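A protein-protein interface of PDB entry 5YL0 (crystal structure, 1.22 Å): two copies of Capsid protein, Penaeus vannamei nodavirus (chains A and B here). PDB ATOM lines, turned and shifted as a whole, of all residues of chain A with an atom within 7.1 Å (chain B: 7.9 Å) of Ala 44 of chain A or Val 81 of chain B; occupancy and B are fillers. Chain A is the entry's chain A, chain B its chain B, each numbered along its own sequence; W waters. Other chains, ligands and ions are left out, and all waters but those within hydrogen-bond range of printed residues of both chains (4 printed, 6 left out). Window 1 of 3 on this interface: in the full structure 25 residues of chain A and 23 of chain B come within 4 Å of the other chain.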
ATOM      1  N   ALA A  13       4.484  24.605 -12.948  1.00  0.00           N
ATOM      2  CA  ALA A  13       3.672  23.437 -12.678  1.00  0.00           C
ATOM      3  C   ALA A  13       2.279  23.727 -13.219  1.00  0.00           C
ATOM      4  O   ALA A  13       1.751  24.859 -12.977  1.00  0.00           O
ATOM      5  CB  ALA A  13       3.653  23.130 -11.211  1.00  0.00           C
ATOM      6  N   VAL A  14       1.660  22.790 -13.879  1.00  0.00           N
ATOM      7  CA  VAL A  14       0.350  22.922 -14.487  1.00  0.00           C
ATOM      8  C   VAL A  14      -0.505  21.742 -14.132  1.00  0.00           C
ATOM      9  O   VAL A  14      -0.022  20.601 -14.110  1.00  0.00           O
ATOM     10  CB  VAL A  14       0.544  23.037 -16.056  1.00  0.00           C
ATOM     11  CG1 VAL A  14      -0.740  23.028 -16.870  1.00  0.00           C
ATOM     12  CG2 VAL A  14       1.262  24.364 -16.407  1.00  0.00           C
ATOM     13  N   ASN A  15      -1.789  21.956 -13.931  1.00  0.00           N
ATOM     14  CA  ASN A  15      -2.751  20.861 -13.729  1.00  0.00           C
ATOM     15  C   ASN A  15      -3.123  20.205 -15.006  1.00  0.00           C
ATOM     16  O   ASN A  15      -3.295  20.829 -16.077  1.00  0.00           O
ATOM     17  CB  ASN A  15      -3.973  21.338 -12.992  1.00  0.00           C
ATOM     18  CG  ASN A  15      -3.677  21.789 -11.584  1.00  0.00           C
ATOM     19  OD1 ASN A  15      -2.728  21.339 -10.969  1.00  0.00           O
ATOM     20  ND2 ASN A  15      -4.484  22.685 -11.096  1.00  0.00           N
ATOM     21  N   PHE A  16      -3.299  18.897 -14.963  1.00  0.00           N
ATOM     22  CA  PHE A  16      -3.966  18.175 -16.076  1.00  0.00           C
ATOM     23  C   PHE A  16      -5.390  18.634 -16.220  1.00  0.00           C
ATOM     24  O   PHE A  16      -6.108  18.863 -15.253  1.00  0.00           O
ATOM     25  CB  PHE A  16      -3.910  16.675 -15.825  1.00  0.00           C
ATOM     26  CG  PHE A  16      -2.597  16.025 -16.090  1.00  0.00           C
ATOM     27  CD1 PHE A  16      -2.058  16.020 -17.358  1.00  0.00           C
ATOM     28  CD2 PHE A  16      -1.893  15.354 -15.111  1.00  0.00           C
ATOM     29  CE1 PHE A  16      -0.885  15.370 -17.622  1.00  0.00           C
ATOM     30  CE2 PHE A  16      -0.673  14.677 -15.371  1.00  0.00           C
ATOM     31  CZ  PHE A  16      -0.180  14.733 -16.625  1.00  0.00           C
ATOM     32  N   THR A  42       6.933  15.625 -15.304  1.00  0.00           N
ATOM     33  CA  THR A  42       6.775  14.521 -14.309  1.00  0.00           C
ATOM     34  C   THR A  42       5.539  14.818 -13.481  1.00  0.00           C
ATOM     35  O   THR A  42       5.181  16.005 -13.302  1.00  0.00           O
ATOM     36  CB  THR A  42       8.003  14.301 -13.389  1.00  0.00           C
ATOM     37  OG1 THR A  42       8.079  15.322 -12.401  1.00  0.00           O
ATOM     38  CG2 THR A  42       9.309  14.317 -14.190  1.00  0.00           C
ATOM     39  N   PRO A  43       4.855  13.833 -12.969  1.00  0.00           N
ATOM     40  CA  PRO A  43       3.551  14.014 -12.308  1.00  0.00           C
ATOM     41  C   PRO A  43       3.675  14.528 -10.898  1.00  0.00           C
ATOM     42  O   PRO A  43       4.618  14.235 -10.168  1.00  0.00           O
ATOM     43  CB  PRO A  43       2.957  12.579 -12.250  1.00  0.00           C
ATOM     44  CG  PRO A  43       4.167  11.717 -12.239  1.00  0.00           C
ATOM     45  CD  PRO A  43       5.157  12.374 -13.164  1.00  0.00           C
ATOM     46  N   ALA A  44       2.663  15.263 -10.455  1.00  0.00           N
ATOM     47  CA  ALA A  44       2.614  15.728  -9.025  1.00  0.00           C
ATOM     48  C   ALA A  44       1.167  16.014  -8.704  1.00  0.00           C
ATOM     49  O   ALA A  44       0.357  16.365  -9.592  1.00  0.00           O
ATOM     50  CB  ALA A  44       3.438  16.926  -8.884  1.00  0.00           C
ATOM     51  N   PHE A  45       0.805  16.011  -7.459  1.00  0.00           N
ATOM     52  CA  PHE A  45      -0.516  16.497  -6.999  1.00  0.00           C
ATOM     53  C   PHE A  45      -0.473  16.705  -5.495  1.00  0.00           C
ATOM     54  O   PHE A  45       0.448  16.210  -4.795  1.00  0.00           O
ATOM     55  CB  PHE A  45      -1.628  15.555  -7.419  1.00  0.00           C
ATOM     56  CG  PHE A  45      -1.439  14.135  -6.947  1.00  0.00           C
ATOM     57  CD1 PHE A  45      -0.982  13.142  -7.852  1.00  0.00           C
ATOM     58  CD2 PHE A  45      -1.699  13.745  -5.681  1.00  0.00           C
ATOM     59  CE1 PHE A  45      -0.816  11.837  -7.430  1.00  0.00           C
ATOM     60  CE2 PHE A  45      -1.512  12.460  -5.250  1.00  0.00           C
ATOM     61  CZ  PHE A  45      -1.066  11.477  -6.128  1.00  0.00           C
ATOM     62  N   LEU A  46      -1.458  17.457  -5.016  1.00  0.00           N
ATOM     63  CA  LEU A  46      -1.449  17.930  -3.619  1.00  0.00           C
ATOM     64  C   LEU A  46      -2.776  17.710  -2.959  1.00  0.00           C
ATOM     65  O   LEU A  46      -3.821  18.213  -3.431  1.00  0.00           O
ATOM     66  CB  LEU A  46      -1.208  19.429  -3.596  1.00  0.00           C
ATOM     67  CG  LEU A  46      -1.086  20.143  -2.266  1.00  0.00           C
ATOM     68  CD1 LEU A  46       0.048  19.529  -1.440  1.00  0.00           C
ATOM     69  CD2 LEU A  46      -0.964  21.625  -2.387  1.00  0.00           C
ATOM     70  N   GLU A  47      -2.763  16.999  -1.850  1.00  0.00           N
ATOM     71  CA  GLU A  47      -3.904  16.904  -0.965  1.00  0.00           C
ATOM     72  C   GLU A  47      -5.157  16.492  -1.646  1.00  0.00           C
ATOM     73  O   GLU A  47      -6.237  17.141  -1.444  1.00  0.00           O
ATOM     74  CB  GLU A  47      -4.076  18.168  -0.152  1.00  0.00           C
ATOM     75  CG  GLU A  47      -2.891  18.492   0.787  1.00  0.00           C
ATOM     76  CD  GLU A  47      -2.926  19.938   1.389  1.00  0.00           C
ATOM     77  OE1 GLU A  47      -2.292  20.176   2.406  1.00  0.00           O
ATOM     78  OE2 GLU A  47      -3.544  20.822   0.861  1.00  0.00           O
ATOM     79  N   ILE A  70       2.888   9.668 -18.905  1.00  0.00           N
ATOM     80  CA  ILE A  70       2.651   9.776 -17.451  1.00  0.00           C
ATOM     81  C   ILE A  70       1.430   8.934 -17.141  1.00  0.00           C
ATOM     82  O   ILE A  70       0.415   9.015 -17.847  1.00  0.00           O
ATOM     83  CB  ILE A  70       2.464  11.259 -17.050  1.00  0.00           C
ATOM     84  CG1 ILE A  70       3.796  11.976 -17.101  1.00  0.00           C
ATOM     85  CG2 ILE A  70       1.801  11.339 -15.674  1.00  0.00           C
ATOM     86  CD1 ILE A  70       3.786  13.477 -16.862  1.00  0.00           C
ATOM     87  N   ILE A  72      -1.084   7.801 -13.840  1.00  0.00           N
ATOM     88  CA  ILE A  72      -1.466   7.961 -12.466  1.00  0.00           C
ATOM     89  C   ILE A  72      -2.659   6.995 -12.230  1.00  0.00           C
ATOM     90  O   ILE A  72      -3.744   7.181 -12.877  1.00  0.00           O
ATOM     91  CB  ILE A  72      -1.928   9.421 -12.145  1.00  0.00           C
ATOM     92  CG1 ILE A  72      -0.784  10.358 -12.306  1.00  0.00           C
ATOM     93  CG2 ILE A  72      -2.497   9.437 -10.701  1.00  0.00           C
ATOM     94  CD1 ILE A  72      -1.120  11.819 -12.183  1.00  0.00           C
ATOM     95  N   MET A  74      -4.718   5.507  -9.071  1.00  0.00           N
ATOM     96  CA  MET A  74      -4.852   5.600  -7.636  1.00  0.00           C
ATOM     97  C   MET A  74      -5.545   4.333  -7.059  1.00  0.00           C
ATOM     98  O   MET A  74      -5.947   4.342  -5.875  1.00  0.00           O
ATOM     99  CB  MET A  74      -5.552   6.894  -7.249  1.00  0.00           C
ATOM    100  CG  MET A  74      -4.721   8.068  -7.724  1.00  0.00           C
ATOM    101  SD  MET A  74      -2.973   8.068  -7.363  1.00  0.00           S
ATOM    102  CE  MET A  74      -2.907   7.991  -5.600  1.00  0.00           C
ATOM    103  N   VAL A  81       2.189   6.367  -9.588  1.00  0.00           N
ATOM    104  CA  VAL A  81       2.355   7.781  -9.966  1.00  0.00           C
ATOM    105  C   VAL A  81       3.677   7.848 -10.640  1.00  0.00           C
ATOM    106  O   VAL A  81       4.719   7.923  -9.946  1.00  0.00           O
ATOM    107  CB  VAL A  81       2.236   8.724  -8.762  1.00  0.00           C
ATOM    108  CG1 VAL A  81       2.409  10.145  -9.243  1.00  0.00           C
ATOM    109  CG2 VAL A  81       0.889   8.544  -8.111  1.00  0.00           C
ATOM    110  N   THR A 109      -7.869  16.707  -8.950  1.00  0.00           N
ATOM    111  CA  THR A 109      -6.921  17.538  -9.627  1.00  0.00           C
ATOM    112  C   THR A 109      -5.524  16.962  -9.511  1.00  0.00           C
ATOM    113  O   THR A 109      -5.008  16.845  -8.374  1.00  0.00           O
ATOM    114  CB  THR A 109      -6.927  18.929  -9.071  1.00  0.00           C
ATOM    115  OG1 THR A 109      -8.234  19.499  -9.196  1.00  0.00           O
ATOM    116  CG2 THR A 109      -6.002  19.860  -9.794  1.00  0.00           C
ATOM    117  N   THR A 110      -4.920  16.679 -10.623  1.00  0.00           N
ATOM    118  CA  THR A 110      -3.524  16.223 -10.627  1.00  0.00           C
ATOM    119  C   THR A 110      -2.774  17.064 -11.654  1.00  0.00           C
ATOM    120  O   THR A 110      -3.429  17.882 -12.385  1.00  0.00           O
ATOM    121  CB  THR A 110      -3.348  14.755 -10.943  1.00  0.00           C
ATOM    122  OG1 THR A 110      -3.637  14.445 -12.295  1.00  0.00           O
ATOM    123  CG2 THR A 110      -4.147  13.904  -9.966  1.00  0.00           C
ATOM    124  N   GLY A 111      -1.483  16.897 -11.853  1.00  0.00           N
ATOM    125  CA  GLY A 111      -0.741  17.807 -12.703  1.00  0.00           C
ATOM    126  C   GLY A 111       0.669  17.346 -12.902  1.00  0.00           C
ATOM    127  O   GLY A 111       1.018  16.181 -12.636  1.00  0.00           O
ATOM    128  N   PHE A 112       1.481  18.249 -13.392  1.00  0.00           N
ATOM    129  CA  PHE A 112       2.858  17.943 -13.762  1.00  0.00           C
ATOM    130  C   PHE A 112       3.747  19.125 -13.583  1.00  0.00           C
ATOM    131  O   PHE A 112       3.348  20.303 -13.683  1.00  0.00           O
ATOM    132  CB  PHE A 112       2.884  17.410 -15.219  1.00  0.00           C
ATOM    133  CG  PHE A 112       2.232  18.257 -16.215  1.00  0.00           C
ATOM    134  CD1 PHE A 112       0.904  18.115 -16.472  1.00  0.00           C
ATOM    135  CD2 PHE A 112       2.975  19.185 -16.972  1.00  0.00           C
ATOM    136  CE1 PHE A 112       0.264  18.939 -17.428  1.00  0.00           C
ATOM    137  CE2 PHE A 112       2.330  19.967 -17.951  1.00  0.00           C
ATOM    138  CZ  PHE A 112       1.023  19.851 -18.155  1.00  0.00           C
ATOM    139  N   ASN A 113       4.987  18.835 -13.302  1.00  0.00           N
ATOM    140  CA  ASN A 113       6.107  19.751 -13.392  1.00  0.00           C
ATOM    141  C   ASN A 113       6.594  19.902 -14.814  1.00  0.00           C
ATOM    142  O   ASN A 113       6.584  18.921 -15.565  1.00  0.00           O
ATOM    143  CB  ASN A 113       7.290  19.175 -12.622  1.00  0.00           C
ATOM    144  CG  ASN A 113       7.017  18.948 -11.197  1.00  0.00           C
ATOM    145  OD1 ASN A 113       6.644  19.922 -10.499  1.00  0.00           O
ATOM    146  ND2 ASN A 113       7.167  17.731 -10.711  1.00  0.00           N
ATOM    147  N   THR B  42      12.918  14.187  -8.879  1.00  0.00           N
ATOM    148  CA  THR B  42      11.485  14.216  -8.810  1.00  0.00           C
ATOM    149  C   THR B  42      10.954  12.843  -8.372  1.00  0.00           C
ATOM    150  O   THR B  42      11.419  11.820  -8.839  1.00  0.00           O
ATOM    151  CB  THR B  42      10.892  14.630 -10.178  1.00  0.00           C
ATOM    152  OG1 THR B  42      11.330  13.759 -11.191  1.00  0.00           O
ATOM    153  CG2 THR B  42      11.246  16.077 -10.567  1.00  0.00           C
ATOM    154  N   PRO B  43       9.871  12.809  -7.610  1.00  0.00           N
ATOM    155  CA  PRO B  43       9.346  11.541  -7.109  1.00  0.00           C
ATOM    156  C   PRO B  43       8.572  10.721  -8.110  1.00  0.00           C
ATOM    157  O   PRO B  43       7.976  11.315  -9.089  1.00  0.00           O
ATOM    158  CB  PRO B  43       8.361  11.994  -5.985  1.00  0.00           C
ATOM    159  CG  PRO B  43       7.955  13.386  -6.326  1.00  0.00           C
ATOM    160  CD  PRO B  43       9.124  13.964  -7.022  1.00  0.00           C
ATOM    161  N   ALA B  44       8.489   9.436  -7.886  1.00  0.00           N
ATOM    162  CA  ALA B  44       7.669   8.524  -8.702  1.00  0.00           C
ATOM    163  C   ALA B  44       7.554   7.194  -7.995  1.00  0.00           C
ATOM    164  O   ALA B  44       8.457   6.859  -7.192  1.00  0.00           O
ATOM    165  CB  ALA B  44       8.290   8.307 -10.064  1.00  0.00           C
ATOM    166  N   PHE B  45       6.544   6.409  -8.263  1.00  0.00           N
ATOM    167  CA  PHE B  45       6.512   5.001  -7.776  1.00  0.00           C
ATOM    168  C   PHE B  45       5.589   4.236  -8.648  1.00  0.00           C
ATOM    169  O   PHE B  45       4.707   4.810  -9.358  1.00  0.00           O
ATOM    170  CB  PHE B  45       6.105   4.911  -6.275  1.00  0.00           C
ATOM    171  CG  PHE B  45       4.795   5.546  -5.974  1.00  0.00           C
ATOM    172  CD1 PHE B  45       4.700   6.816  -5.405  1.00  0.00           C
ATOM    173  CD2 PHE B  45       3.600   4.891  -6.246  1.00  0.00           C
ATOM    174  CE1 PHE B  45       3.467   7.340  -5.112  1.00  0.00           C
ATOM    175  CE2 PHE B  45       2.389   5.464  -6.005  1.00  0.00           C
ATOM    176  CZ  PHE B  45       2.346   6.666  -5.431  1.00  0.00           C
ATOM    177  N   PHE B  50       0.002   0.326  -0.724  1.00  0.00           N
ATOM    178  CA  PHE B  50       0.216   1.058   0.493  1.00  0.00           C
ATOM    179  C   PHE B  50      -0.709   0.672   1.667  1.00  0.00           C
ATOM    180  O   PHE B  50      -0.450   1.159   2.781  1.00  0.00           O
ATOM    181  CB  PHE B  50       0.191   2.534   0.265  1.00  0.00           C
ATOM    182  CG  PHE B  50       1.267   3.062  -0.689  1.00  0.00           C
ATOM    183  CD1 PHE B  50       2.582   3.213  -0.296  1.00  0.00           C
ATOM    184  CD2 PHE B  50       0.878   3.456  -1.961  1.00  0.00           C
ATOM    185  CE1 PHE B  50       3.496   3.692  -1.189  1.00  0.00           C
ATOM    186  CE2 PHE B  50       1.810   3.954  -2.800  1.00  0.00           C
ATOM    187  CZ  PHE B  50       3.081   4.144  -2.430  1.00  0.00           C
ATOM    188  N   ILE B  70      10.937  16.600  -1.163  1.00  0.00           N
ATOM    189  CA  ILE B  70      10.004  15.695  -1.834  1.00  0.00           C
ATOM    190  C   ILE B  70       9.085  15.169  -0.777  1.00  0.00           C
ATOM    191  O   ILE B  70       9.579  14.749   0.319  1.00  0.00           O
ATOM    192  CB  ILE B  70      10.778  14.558  -2.551  1.00  0.00           C
ATOM    193  CG1 ILE B  70      11.385  15.142  -3.822  1.00  0.00           C
ATOM    194  CG2 ILE B  70       9.898  13.385  -2.796  1.00  0.00           C
ATOM    195  CD1 ILE B  70      12.337  14.251  -4.550  1.00  0.00           C
ATOM    196  N   SER B  71       7.779  15.074  -1.039  1.00  0.00           N
ATOM    197  CA  SER B  71       6.793  14.536  -0.140  1.00  0.00           C
ATOM    198  C   SER B  71       5.970  13.477  -0.879  1.00  0.00           C
ATOM    199  O   SER B  71       5.411  13.731  -1.976  1.00  0.00           O
ATOM    200  CB  SER B  71       5.846  15.727   0.201  1.00  0.00           C
ATOM    201  OG  SER B  71       6.491  16.780   0.817  1.00  0.00           O
ATOM    202  N   ILE B  72       5.847  12.329  -0.243  1.00  0.00           N
ATOM    203  CA  ILE B  72       4.912  11.308  -0.708  1.00  0.00           C
ATOM    204  C   ILE B  72       4.062  10.909   0.481  1.00  0.00           C
ATOM    205  O   ILE B  72       4.573  10.313   1.468  1.00  0.00           O
ATOM    206  CB  ILE B  72       5.661  10.081  -1.192  1.00  0.00           C
ATOM    207  CG1 ILE B  72       6.545  10.422  -2.423  1.00  0.00           C
ATOM    208  CG2 ILE B  72       4.586   9.048  -1.644  1.00  0.00           C
ATOM    209  CD1 ILE B  72       7.448   9.281  -2.900  1.00  0.00           C
ATOM    210  N   ASN B  73       2.834  11.304   0.542  1.00  0.00           N
ATOM    211  CA  ASN B  73       1.910  11.068   1.628  1.00  0.00           C
ATOM    212  C   ASN B  73       0.716  10.342   1.108  1.00  0.00           C
ATOM    213  O   ASN B  73      -0.121  10.904   0.363  1.00  0.00           O
ATOM    214  CB  ASN B  73       1.458  12.403   2.310  1.00  0.00           C
ATOM    215  CG  ASN B  73       0.624  12.123   3.516  1.00  0.00           C
ATOM    216  OD1 ASN B  73      -0.109  11.183   3.604  1.00  0.00           O
ATOM    217  ND2 ASN B  73       0.841  13.000   4.561  1.00  0.00           N
ATOM    218  N   MET B  74       0.575   9.055   1.476  1.00  0.00           N
ATOM    219  CA  MET B  74      -0.434   8.198   0.939  1.00  0.00           C
ATOM    220  C   MET B  74      -1.656   8.104   1.860  1.00  0.00           C
ATOM    221  O   MET B  74      -2.460   7.187   1.733  1.00  0.00           O
ATOM    222  CB  MET B  74       0.125   6.812   0.640  1.00  0.00           C
ATOM    223  CG  MET B  74       1.295   6.919  -0.436  1.00  0.00           C
ATOM    224  SD  MET B  74       0.960   7.907  -1.872  1.00  0.00           S
ATOM    225  CE  MET B  74      -0.095   7.140  -2.414  1.00  0.00           C
ATOM    226  N   VAL B  78      -6.235  12.364   1.860  1.00  0.00           N
ATOM    227  CA  VAL B  78      -5.466  13.505   1.628  1.00  0.00           C
ATOM    228  C   VAL B  78      -4.097  13.084   1.059  1.00  0.00           C
ATOM    229  O   VAL B  78      -3.094  13.003   1.783  1.00  0.00           O
ATOM    230  CB  VAL B  78      -5.280  14.313   2.951  1.00  0.00           C
ATOM    231  CG1 VAL B  78      -4.631  15.610   2.614  1.00  0.00           C
ATOM    232  CG2 VAL B  78      -6.572  14.455   3.751  1.00  0.00           C
ATOM    233  N   THR B  79      -4.060  12.793  -0.224  1.00  0.00           N
ATOM    234  CA  THR B  79      -2.901  12.130  -0.845  1.00  0.00           C
ATOM    235  C   THR B  79      -2.095  13.148  -1.564  1.00  0.00           C
ATOM    236  O   THR B  79      -2.637  13.938  -2.342  1.00  0.00           O
ATOM    237  CB  THR B  79      -3.447  11.063  -1.817  1.00  0.00           C
ATOM    238  OG1 THR B  79      -4.459  10.301  -1.170  1.00  0.00           O
ATOM    239  CG2 THR B  79      -2.339  10.176  -2.329  1.00  0.00           C
ATOM    240  N   THR B  80      -0.770  13.093  -1.421  1.00  0.00           N
ATOM    241  CA  THR B  80       0.150  14.044  -2.015  1.00  0.00           C
ATOM    242  C   THR B  80       1.323  13.343  -2.617  1.00  0.00           C
ATOM    243  O   THR B  80       1.954  12.451  -1.934  1.00  0.00           O
ATOM    244  CB  THR B  80       0.669  15.044  -0.960  1.00  0.00           C
ATOM    245  OG1 THR B  80      -0.467  15.810  -0.520  1.00  0.00           O
ATOM    246  CG2 THR B  80       1.691  15.986  -1.466  1.00  0.00           C
ATOM    247  N   VAL B  81       1.731  13.720  -3.819  1.00  0.00           N
ATOM    248  CA  VAL B  81       3.081  13.340  -4.366  1.00  0.00           C
ATOM    249  C   VAL B  81       3.629  14.590  -4.935  1.00  0.00           C
ATOM    250  O   VAL B  81       3.098  15.091  -5.977  1.00  0.00           O
ATOM    251  CB  VAL B  81       2.918  12.248  -5.447  1.00  0.00           C
ATOM    252  CG1 VAL B  81       4.277  11.949  -6.065  1.00  0.00           C
ATOM    253  CG2 VAL B  81       2.359  10.986  -4.877  1.00  0.00           C
ATOM    254  N   SER B  82       4.626  15.224  -4.313  1.00  0.00           N
ATOM    255  CA  SER B  82       4.972  16.592  -4.712  1.00  0.00           C
ATOM    256  C   SER B  82       6.427  16.875  -4.428  1.00  0.00           C
ATOM    257  O   SER B  82       7.147  16.113  -3.708  1.00  0.00           O
ATOM    258  CB  SER B  82       4.103  17.587  -3.868  1.00  0.00           C
ATOM    259  OG  SER B  82       4.520  17.595  -2.552  1.00  0.00           O
ATOM    260  N   GLY B  83       6.860  18.000  -4.932  1.00  0.00           N
ATOM    261  CA  GLY B  83       8.131  18.539  -4.673  1.00  0.00           C
ATOM    262  C   GLY B  83       9.238  17.991  -5.556  1.00  0.00           C
ATOM    263  O   GLY B  83       9.056  17.270  -6.528  1.00  0.00           O
ATOM    264  N   PHE B  84      10.409  18.486  -5.245  1.00  0.00           N
ATOM    265  CA  PHE B  84      11.642  18.197  -5.982  1.00  0.00           C
ATOM    266  C   PHE B  84      12.822  18.514  -5.127  1.00  0.00           C
ATOM    267  O   PHE B  84      12.703  19.199  -4.120  1.00  0.00           O
ATOM    268  CB  PHE B  84      11.709  18.998  -7.268  1.00  0.00           C
ATOM    269  CG  PHE B  84      11.678  20.499  -7.010  1.00  0.00           C
ATOM    270  CD1 PHE B  84      12.799  21.218  -6.619  1.00  0.00           C
ATOM    271  CD2 PHE B  84      10.454  21.178  -7.080  1.00  0.00           C
ATOM    272  CE1 PHE B  84      12.727  22.573  -6.315  1.00  0.00           C
ATOM    273  CE2 PHE B  84      10.395  22.526  -6.876  1.00  0.00           C
ATOM    274  CZ  PHE B  84      11.491  23.229  -6.418  1.00  0.00           C
ATOM    275  N   THR B 110       9.247   3.374  -3.073  1.00  0.00           N
ATOM    276  CA  THR B 110       9.090   4.569  -3.861  1.00  0.00           C
ATOM    277  C   THR B 110      10.403   5.084  -4.324  1.00  0.00           C
ATOM    278  O   THR B 110      11.447   4.504  -3.904  1.00  0.00           O
ATOM    279  CB  THR B 110       8.278   5.647  -3.128  1.00  0.00           C
ATOM    280  OG1 THR B 110       9.093   6.201  -2.123  1.00  0.00           O
ATOM    281  CG2 THR B 110       6.931   5.196  -2.612  1.00  0.00           C
ATOM    282  N   GLY B 111      10.471   6.115  -5.184  1.00  0.00           N
ATOM    283  CA  GLY B 111      11.771   6.487  -5.740  1.00  0.00           C
ATOM    284  C   GLY B 111      11.698   7.846  -6.402  1.00  0.00           C
ATOM    285  O   GLY B 111      10.734   8.619  -6.213  1.00  0.00           O
HETATM  286  O   HOH W   1       5.412  14.517  -7.672  1.00  0.00           O
HETATM  287  O   HOH W   2       7.311  13.986  -9.978  1.00  0.00           O
HETATM  288  O   HOH W   3       2.414  13.044  -8.037  1.00  0.00           O
HETATM  289  O   HOH W   4       6.047  10.187 -10.743  1.00  0.00           O
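The backbone NH of Phe 45 of chain A lies within hydrogen-bond range of the backbone carbonyl oxygen of Val 81 of chain B (2.9 Å).
O of Thr 79 of chain B sits at hydrogen-bond distance from N of Glu 47 of chain A (3.1 Å).
The backbone NH (N) of Glu 47 of chain A lies within hydrogen-bond range of the side-chain hydroxyl (OG1) of Thr 80 of chain B, 2.9 Å away.
O of Val 81 of chain A is in hydrogen-bond range of N of Phe 45 of chain B.
The backbone carbonyl oxygen of Thr 42 of chain A lies within hydrogen-bond range of the backbone NH of Asn 113 of chain A (2.8 Å).
O of Gly 111 of chain A sits at hydrogen-bond distance from N of Ala 44 of chain A (2.9 Å).
O of Gly 111 of chain B is in hydrogen-bond range of N of Ala 44 of chain B, at 2.9 Å.
N of Asn 73 of chain B is in hydrogen-bond range of O of Thr 80 of chain B.
Among the printed residues, pairs that only touch across the chains: Ala 44 of chain A with Val 81 of chain B, Val 81 of chain A with Ala 44 of chain B, Phe 45 of chain A with Thr 79 of chain B, Phe 45 of chain A with Thr 80 of chain B, Thr 42 of chain A with Thr 42 of chain B, Glu 47 of chain A with Val 78 of chain B, Leu 46 of chain A with Thr 79 of chain B, Leu 46 of chain A with Thr 80 of chain B and Met 74 of chain A with Thr 79 of chain B.
Of the printed residues of chain B, Thr 42 of chain A touches Thr 42 (3.7 Å).
Ala 44 of chain A touches just one residue of chain B: Val 81 (3.2 Å).
Of the printed residues of chain B, Phe 45 of chain A touches Thr 79, Thr 80 and Val 81.
Of the printed residues of chain B, Leu 46 of chain A touches Thr 79 and Thr 80.
No residue of chain B comes within 4 Å of Gly 111 of chain A.
Of the printed residues of chain A, Ala 44 of chain B touches Val 81 (3.3 Å).
Ser 71 of chain B touches none of the printed residues of chain A.
Of chain A, only Ala 44 and Phe 45 come within 4 Å of Val 81 of chain B.
The nearest residue of chain A that does not touch Val 81 of chain B is Val 81 of chain A (4.1 Å).
The nearest printed residue of chain B that does not touch Val 81 of chain A is Val 81 of chain B (4.1 Å).
Printed residues of chain B that touch a printed residue of chain A: Thr 42, Ala 44, Phe 45, Val 78, Thr 79, Thr 80 and Val 81.
Along chain B the printed residues that touch a printed residue of chain A span positions 42 to 81.
Hydrophobic or aromatic side chains of chain A that line the printed part of chain B: Ala 44, Phe 45, Leu 46, Met 74 and Val 81.
Thr 42 of chain A touches its own counterpart, Thr 42 of chain B.
Ala 44 of chain A touches Val 81 of chain B, and with the chains exchanged Val 81 of chain A touches Ala 44 of chain B.
Phe 45 of chain A touches Val 81 of chain B, and with the chains exchanged Val 81 of chain A touches Phe 45 of chain B.
10 positions are printed for both chains.
Of the 13 pairs that touch across the chains among the printed residues, 5 have their exchanged pair printed and touching as well.
Water W1 lies within hydrogen-bond range of O of Pro 43 of chain A (2.6 Å) and O of Val 81 of chain B (2.9 Å).
Water W2 lies within hydrogen-bond range of the backbone carbonyl oxygen of Pro 43 of chain A (2.7 Å), the side-chain hydroxyl of Thr 42 of chain A (2.9 Å) and the backbone carbonyl oxygen of Pro 43 of chain B (2.9 Å).
Water W4 lies within hydrogen-bond range of the backbone carbonyl oxygen of Val 81 of chain A (2.7 Å) and the backbone carbonyl oxygen of Pro 43 of chain B (2.8 Å).
Water W3 lies within hydrogen-bond range of the backbone carbonyl oxygen of Val 81 of chain B (3.0 Å), the backbone carbonyl oxygen of Pro 43 of chain A (3.3 Å), the backbone NH of Ala 44 of chain A (3.3 Å) and the backbone NH of Phe 45 of chain A (3.4 Å).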
